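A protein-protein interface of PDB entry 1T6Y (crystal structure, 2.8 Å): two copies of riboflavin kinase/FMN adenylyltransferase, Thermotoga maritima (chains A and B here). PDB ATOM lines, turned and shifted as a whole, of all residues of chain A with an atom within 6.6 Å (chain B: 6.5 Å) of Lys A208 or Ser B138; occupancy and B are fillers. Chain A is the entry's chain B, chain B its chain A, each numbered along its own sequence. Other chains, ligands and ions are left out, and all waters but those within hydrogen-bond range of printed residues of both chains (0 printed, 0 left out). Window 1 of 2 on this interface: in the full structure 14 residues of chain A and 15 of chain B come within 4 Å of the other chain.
Of the printed residues of chain B, Asp A206 touches Ser B136 and Leu B139. Of chain B, only Ser B136 (3.9 Å) and Ser B138 (3.2 Å) come within 4 Å of Lys A208. Pro B50 touches none of the printed residues of chain A. Of chain A, only Gly A207 and Lys A208 come within 4 Å of Ser B138. Printed residues of chain A within 4 Å of Asn B142: Gly A207 (3.8 Å). Leu B143 touches none of the printed residues of chain A. The nearest residue of chain B that does not touch Lys A208 is Ser B137 (5.1 Å). The nearest printed residue of chain B that does not touch Asp A206 is Asn B142 (4.4 Å).
Printed residues of chain A that touch a printed residue of chain B: Asp A206, Gly A207 and Lys A208. Along chain A the printed residues that touch a printed residue of chain B span positions 206 to 208.
The side-chain hydroxyl (OG) of Ser B136 lies within hydrogen-bond range of the side-chain carboxylate (OD2) of Asp A206 (3.4 Å).
Leu B139 touches Asp A206 (CD1 to OD1, 2.8 Å). Ser B138 touches Gly A207. CA of Gly A207 touches ND2 of Asn B142 (3.8 Å). Lys A208 touches Ser B136. Ser B138 touches Lys A208 (OG to CD, 3.2 Å).
A ring nitrogen (NE2) of His B12 sits close to the backbone NH (N) of Ser B136, at 3.4 Å. OG of Ser B136 sits at hydrogen-bond distance from N of Leu B139 (3.0 Å).
No position is printed for both chains. Of the 6 pairs that touch across the chains among the printed residues, none has its exchanged pair printed and touching as well.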
ATOM      1  N   VAL A 202      -0.088 -29.979   4.192  1.00  0.00           N
ATOM      2  CA  VAL A 202       1.371 -30.104   4.182  1.00  0.00           C
ATOM      3  C   VAL A 202       2.095 -29.521   5.406  1.00  0.00           C
ATOM      4  O   VAL A 202       1.677 -28.514   5.963  1.00  0.00           O
ATOM      5  CB  VAL A 202       1.954 -29.449   2.885  1.00  0.00           C
ATOM      6  CG1 VAL A 202       3.403 -29.847   2.691  1.00  0.00           C
ATOM      7  CG2 VAL A 202       1.135 -29.854   1.671  1.00  0.00           C
ATOM      8  N   HIS A 203       3.175 -30.184   5.818  1.00  0.00           N
ATOM      9  CA  HIS A 203       4.007 -29.759   6.947  1.00  0.00           C
ATOM     10  C   HIS A 203       5.388 -29.510   6.322  1.00  0.00           C
ATOM     11  O   HIS A 203       6.196 -30.434   6.161  1.00  0.00           O
ATOM     12  CB  HIS A 203       4.095 -30.864   8.021  1.00  0.00           C
ATOM     13  CG  HIS A 203       4.533 -30.373   9.371  1.00  0.00           C
ATOM     14  ND1 HIS A 203       5.680 -29.633   9.563  1.00  0.00           N
ATOM     15  CD2 HIS A 203       3.974 -30.519  10.597  1.00  0.00           C
ATOM     16  CE1 HIS A 203       5.809 -29.344  10.846  1.00  0.00           C
ATOM     17  NE2 HIS A 203       4.786 -29.869  11.495  1.00  0.00           N
ATOM     18  N   LEU A 204       5.628 -28.249   5.954  1.00  0.00           N
ATOM     19  CA  LEU A 204       6.872 -27.819   5.318  1.00  0.00           C
ATOM     20  C   LEU A 204       8.056 -27.824   6.273  1.00  0.00           C
ATOM     21  O   LEU A 204       7.898 -27.587   7.474  1.00  0.00           O
ATOM     22  CB  LEU A 204       6.696 -26.414   4.729  1.00  0.00           C
ATOM     23  CG  LEU A 204       5.796 -26.213   3.504  1.00  0.00           C
ATOM     24  CD1 LEU A 204       5.442 -24.743   3.408  1.00  0.00           C
ATOM     25  CD2 LEU A 204       6.496 -26.681   2.227  1.00  0.00           C
ATOM     26  N   PRO A 205       9.262 -28.092   5.736  1.00  0.00           N
ATOM     27  CA  PRO A 205      10.539 -28.150   6.459  1.00  0.00           C
ATOM     28  C   PRO A 205      10.700 -26.969   7.396  1.00  0.00           C
ATOM     29  O   PRO A 205      10.968 -27.139   8.588  1.00  0.00           O
ATOM     30  CB  PRO A 205      11.573 -28.138   5.335  1.00  0.00           C
ATOM     31  CG  PRO A 205      10.887 -28.916   4.263  1.00  0.00           C
ATOM     32  CD  PRO A 205       9.466 -28.374   4.301  1.00  0.00           C
ATOM     33  N   ASP A 206      10.551 -25.768   6.844  1.00  0.00           N
ATOM     34  CA  ASP A 206      10.661 -24.561   7.640  1.00  0.00           C
ATOM     35  C   ASP A 206       9.766 -24.717   8.862  1.00  0.00           C
ATOM     36  O   ASP A 206      10.251 -24.751   9.996  1.00  0.00           O
ATOM     37  CB  ASP A 206      10.223 -23.345   6.824  1.00  0.00           C
ATOM     38  CG  ASP A 206       9.953 -22.133   7.695  1.00  0.00           C
ATOM     39  OD1 ASP A 206      10.773 -21.868   8.595  1.00  0.00           O
ATOM     40  OD2 ASP A 206       8.929 -21.446   7.484  1.00  0.00           O
ATOM     41  N   GLY A 207       8.461 -24.831   8.616  1.00  0.00           N
ATOM     42  CA  GLY A 207       7.507 -24.987   9.698  1.00  0.00           C
ATOM     43  C   GLY A 207       6.101 -24.569   9.313  1.00  0.00           C
ATOM     44  O   GLY A 207       5.162 -24.760  10.084  1.00  0.00           O
ATOM     45  N   LYS A 208       5.945 -24.007   8.120  1.00  0.00           N
ATOM     46  CA  LYS A 208       4.635 -23.562   7.663  1.00  0.00           C
ATOM     47  C   LYS A 208       3.775 -24.755   7.257  1.00  0.00           C
ATOM     48  O   LYS A 208       4.289 -25.777   6.799  1.00  0.00           O
ATOM     49  CB  LYS A 208       4.784 -22.621   6.457  1.00  0.00           C
ATOM     50  CG  LYS A 208       4.003 -21.299   6.537  1.00  0.00           C
ATOM     51  CD  LYS A 208       4.730 -20.271   7.407  1.00  0.00           C
ATOM     52  CE  LYS A 208       4.139 -18.861   7.295  1.00  0.00           C
ATOM     53  NZ  LYS A 208       4.346 -18.244   5.951  1.00  0.00           N
ATOM     54  N   LYS A 209       2.462 -24.605   7.412  1.00  0.00           N
ATOM     55  CA  LYS A 209       1.505 -25.644   7.056  1.00  0.00           C
ATOM     56  C   LYS A 209       0.527 -25.159   5.977  1.00  0.00           C
ATOM     57  O   LYS A 209      -0.470 -24.479   6.273  1.00  0.00           O
ATOM     58  CB  LYS A 209       0.714 -26.086   8.299  1.00  0.00           C
ATOM     59  CG  LYS A 209       0.951 -27.535   8.729  1.00  0.00           C
ATOM     60  CD  LYS A 209      -0.018 -27.965   9.832  1.00  0.00           C
ATOM     61  CE  LYS A 209       0.300 -29.360  10.374  1.00  0.00           C
ATOM     62  NZ  LYS A 209       0.248 -30.437   9.326  1.00  0.00           N
ATOM     63  N   LYS A 210       0.795 -25.535   4.731  1.00  0.00           N
ATOM     64  CA  LYS A 210      -0.056 -25.123   3.618  1.00  0.00           C
ATOM     65  C   LYS A 210      -0.939 -26.258   3.124  1.00  0.00           C
ATOM     66  O   LYS A 210      -0.524 -27.405   3.121  1.00  0.00           O
ATOM     67  CB  LYS A 210       0.815 -24.646   2.445  1.00  0.00           C
ATOM     68  CG  LYS A 210       1.769 -23.495   2.760  1.00  0.00           C
ATOM     69  CD  LYS A 210       1.289 -22.175   2.149  1.00  0.00           C
ATOM     70  CE  LYS A 210       2.249 -21.029   2.452  1.00  0.00           C
ATOM     71  NZ  LYS A 210       3.621 -21.308   1.943  1.00  0.00           N
ATOM     72  N   PHE A 237       2.344 -21.379  -2.784  1.00  0.00           N
ATOM     73  CA  PHE A 237       3.686 -21.652  -2.290  1.00  0.00           C
ATOM     74  C   PHE A 237       4.638 -21.711  -3.462  1.00  0.00           C
ATOM     75  O   PHE A 237       4.246 -22.065  -4.581  1.00  0.00           O
ATOM     76  CB  PHE A 237       3.703 -23.011  -1.532  1.00  0.00           C
ATOM     77  CG  PHE A 237       5.085 -23.461  -1.078  1.00  0.00           C
ATOM     78  CD1 PHE A 237       5.629 -23.003   0.124  1.00  0.00           C
ATOM     79  CD2 PHE A 237       5.862 -24.292  -1.893  1.00  0.00           C
ATOM     80  CE1 PHE A 237       6.931 -23.356   0.506  1.00  0.00           C
ATOM     81  CE2 PHE A 237       7.158 -24.652  -1.528  1.00  0.00           C
ATOM     82  CZ  PHE A 237       7.700 -24.183  -0.325  1.00  0.00           C
ATOM     83  N   HIS B  12       8.372 -10.050  13.086  1.00  0.00           N
ATOM     84  CA  HIS B  12       9.726 -10.485  12.932  1.00  0.00           C
ATOM     85  C   HIS B  12      10.580  -9.655  11.984  1.00  0.00           C
ATOM     86  O   HIS B  12      10.178  -8.600  11.489  1.00  0.00           O
ATOM     87  CB  HIS B  12       9.793 -11.960  12.543  1.00  0.00           C
ATOM     88  CG  HIS B  12       9.014 -12.338  11.324  1.00  0.00           C
ATOM     89  ND1 HIS B  12       7.680 -12.678  11.374  1.00  0.00           N
ATOM     90  CD2 HIS B  12       9.426 -12.638  10.069  1.00  0.00           C
ATOM     91  CE1 HIS B  12       7.308 -13.191  10.212  1.00  0.00           C
ATOM     92  NE2 HIS B  12       8.350 -13.180   9.402  1.00  0.00           N
ATOM     93  N   PRO B  50      -0.367 -23.792  16.520  1.00  0.00           N
ATOM     94  CA  PRO B  50       0.533 -23.539  17.647  1.00  0.00           C
ATOM     95  C   PRO B  50       0.061 -22.417  18.533  1.00  0.00           C
ATOM     96  O   PRO B  50      -0.250 -22.631  19.685  1.00  0.00           O
ATOM     97  CB  PRO B  50       1.854 -23.210  16.970  1.00  0.00           C
ATOM     98  CG  PRO B  50       1.835 -24.095  15.783  1.00  0.00           C
ATOM     99  CD  PRO B  50       0.399 -23.955  15.272  1.00  0.00           C
ATOM    100  N   LEU B  53       2.411 -15.437  18.780  1.00  0.00           N
ATOM    101  CA  LEU B  53       3.564 -15.161  19.606  1.00  0.00           C
ATOM    102  C   LEU B  53       3.320 -14.005  20.574  1.00  0.00           C
ATOM    103  O   LEU B  53       4.120 -13.776  21.480  1.00  0.00           O
ATOM    104  CB  LEU B  53       4.779 -14.868  18.733  1.00  0.00           C
ATOM    105  CG  LEU B  53       5.140 -15.937  17.714  1.00  0.00           C
ATOM    106  CD1 LEU B  53       4.273 -15.757  16.527  1.00  0.00           C
ATOM    107  CD2 LEU B  53       6.580 -15.824  17.308  1.00  0.00           C
ATOM    108  N   ASP B 101       4.701 -13.792  -1.095  1.00  0.00           N
ATOM    109  CA  ASP B 101       3.593 -14.700  -0.865  1.00  0.00           C
ATOM    110  C   ASP B 101       2.223 -14.031  -0.899  1.00  0.00           C
ATOM    111  O   ASP B 101       1.329 -14.467  -1.624  1.00  0.00           O
ATOM    112  CB  ASP B 101       3.797 -15.441   0.467  1.00  0.00           C
ATOM    113  CG  ASP B 101       4.634 -14.645   1.469  1.00  0.00           C
ATOM    114  OD1 ASP B 101       5.819 -14.990   1.707  1.00  0.00           O
ATOM    115  OD2 ASP B 101       4.106 -13.664   2.022  1.00  0.00           O
ATOM    116  N   VAL B 135      12.253 -16.369   7.159  1.00  0.00           N
ATOM    117  CA  VAL B 135      11.672 -15.986   8.445  1.00  0.00           C
ATOM    118  C   VAL B 135      10.135 -16.017   8.374  1.00  0.00           C
ATOM    119  O   VAL B 135       9.532 -15.733   7.324  1.00  0.00           O
ATOM    120  CB  VAL B 135      12.103 -14.577   8.867  1.00  0.00           C
ATOM    121  CG1 VAL B 135      11.990 -14.443  10.372  1.00  0.00           C
ATOM    122  CG2 VAL B 135      13.527 -14.294   8.426  1.00  0.00           C
ATOM    123  N   SER B 136       9.491 -16.382   9.474  1.00  0.00           N
ATOM    124  CA  SER B 136       8.038 -16.455   9.487  1.00  0.00           C
ATOM    125  C   SER B 136       7.584 -16.639  10.894  1.00  0.00           C
ATOM    126  O   SER B 136       8.370 -17.056  11.734  1.00  0.00           O
ATOM    127  CB  SER B 136       7.559 -17.646   8.701  1.00  0.00           C
ATOM    128  OG  SER B 136       8.052 -18.784   9.338  1.00  0.00           O
ATOM    129  N   SER B 137       6.316 -16.330  11.153  1.00  0.00           N
ATOM    130  CA  SER B 137       5.748 -16.481  12.484  1.00  0.00           C
ATOM    131  C   SER B 137       5.767 -17.968  12.818  1.00  0.00           C
ATOM    132  O   SER B 137       6.052 -18.335  13.955  1.00  0.00           O
ATOM    133  CB  SER B 137       4.325 -15.925  12.527  1.00  0.00           C
ATOM    134  OG  SER B 137       4.325 -14.506  12.490  1.00  0.00           O
ATOM    135  N   SER B 138       5.491 -18.810  11.814  1.00  0.00           N
ATOM    136  CA  SER B 138       5.519 -20.274  11.966  1.00  0.00           C
ATOM    137  C   SER B 138       6.835 -20.757  12.568  1.00  0.00           C
ATOM    138  O   SER B 138       6.894 -21.301  13.664  1.00  0.00           O
ATOM    139  CB  SER B 138       5.365 -20.957  10.613  1.00  0.00           C
ATOM    140  OG  SER B 138       4.013 -21.262  10.345  1.00  0.00           O
ATOM    141  N   LEU B 139       7.887 -20.570  11.802  1.00  0.00           N
ATOM    142  CA  LEU B 139       9.217 -20.930  12.214  1.00  0.00           C
ATOM    143  C   LEU B 139       9.547 -20.498  13.642  1.00  0.00           C
ATOM    144  O   LEU B 139      10.230 -21.213  14.361  1.00  0.00           O
ATOM    145  CB  LEU B 139      10.217 -20.299  11.234  1.00  0.00           C
ATOM    146  CG  LEU B 139      11.726 -20.511  11.359  1.00  0.00           C
ATOM    147  CD1 LEU B 139      12.349 -20.115  10.053  1.00  0.00           C
ATOM    148  CD2 LEU B 139      12.323 -19.690  12.480  1.00  0.00           C
ATOM    149  N   ILE B 140       9.092 -19.329  14.062  1.00  0.00           N
ATOM    150  CA  ILE B 140       9.437 -18.889  15.412  1.00  0.00           C
ATOM    151  C   ILE B 140       8.504 -19.567  16.393  1.00  0.00           C
ATOM    152  O   ILE B 140       8.893 -19.900  17.517  1.00  0.00           O
ATOM    153  CB  ILE B 140       9.318 -17.339  15.555  1.00  0.00           C
ATOM    154  CG1 ILE B 140      10.115 -16.658  14.447  1.00  0.00           C
ATOM    155  CG2 ILE B 140       9.862 -16.882  16.897  1.00  0.00           C
ATOM    156  CD1 ILE B 140      10.023 -15.142  14.478  1.00  0.00           C
ATOM    157  N   ARG B 141       7.266 -19.752  15.932  1.00  0.00           N
ATOM    158  CA  ARG B 141       6.186 -20.384  16.677  1.00  0.00           C
ATOM    159  C   ARG B 141       6.659 -21.780  17.162  1.00  0.00           C
ATOM    160  O   ARG B 141       6.200 -22.288  18.190  1.00  0.00           O
ATOM    161  CB  ARG B 141       4.949 -20.501  15.750  1.00  0.00           C
ATOM    162  CG  ARG B 141       3.623 -19.899  16.291  1.00  0.00           C
ATOM    163  CD  ARG B 141       3.167 -18.584  15.622  1.00  0.00           C
ATOM    164  NE  ARG B 141       2.216 -18.752  14.514  1.00  0.00           N
ATOM    165  CZ  ARG B 141       1.565 -17.759  13.881  1.00  0.00           C
ATOM    166  NH1 ARG B 141       1.727 -16.485  14.221  1.00  0.00           N
ATOM    167  NH2 ARG B 141       0.753 -18.042  12.866  1.00  0.00           N
ATOM    168  N   ASN B 142       7.590 -22.387  16.432  1.00  0.00           N
ATOM    169  CA  ASN B 142       8.096 -23.693  16.807  1.00  0.00           C
ATOM    170  C   ASN B 142       9.223 -23.667  17.828  1.00  0.00           C
ATOM    171  O   ASN B 142       9.113 -24.281  18.886  1.00  0.00           O
ATOM    172  CB  ASN B 142       8.527 -24.459  15.572  1.00  0.00           C
ATOM    173  CG  ASN B 142       7.346 -24.944  14.772  1.00  0.00           C
ATOM    174  OD1 ASN B 142       6.320 -25.315  15.340  1.00  0.00           O
ATOM    175  ND2 ASN B 142       7.477 -24.960  13.452  1.00  0.00           N
ATOM    176  N   LEU B 143      10.315 -22.978  17.517  1.00  0.00           N
ATOM    177  CA  LEU B 143      11.420 -22.890  18.464  1.00  0.00           C
ATOM    178  C   LEU B 143      10.850 -22.633  19.871  1.00  0.00           C
ATOM    179  O   LEU B 143      11.380 -23.122  20.868  1.00  0.00           O
ATOM    180  CB  LEU B 143      12.349 -21.734  18.073  1.00  0.00           C
ATOM    181  CG  LEU B 143      12.689 -21.738  16.588  1.00  0.00           C
ATOM    182  CD1 LEU B 143      13.212 -20.370  16.147  1.00  0.00           C
ATOM    183  CD2 LEU B 143      13.697 -22.828  16.332  1.00  0.00           C
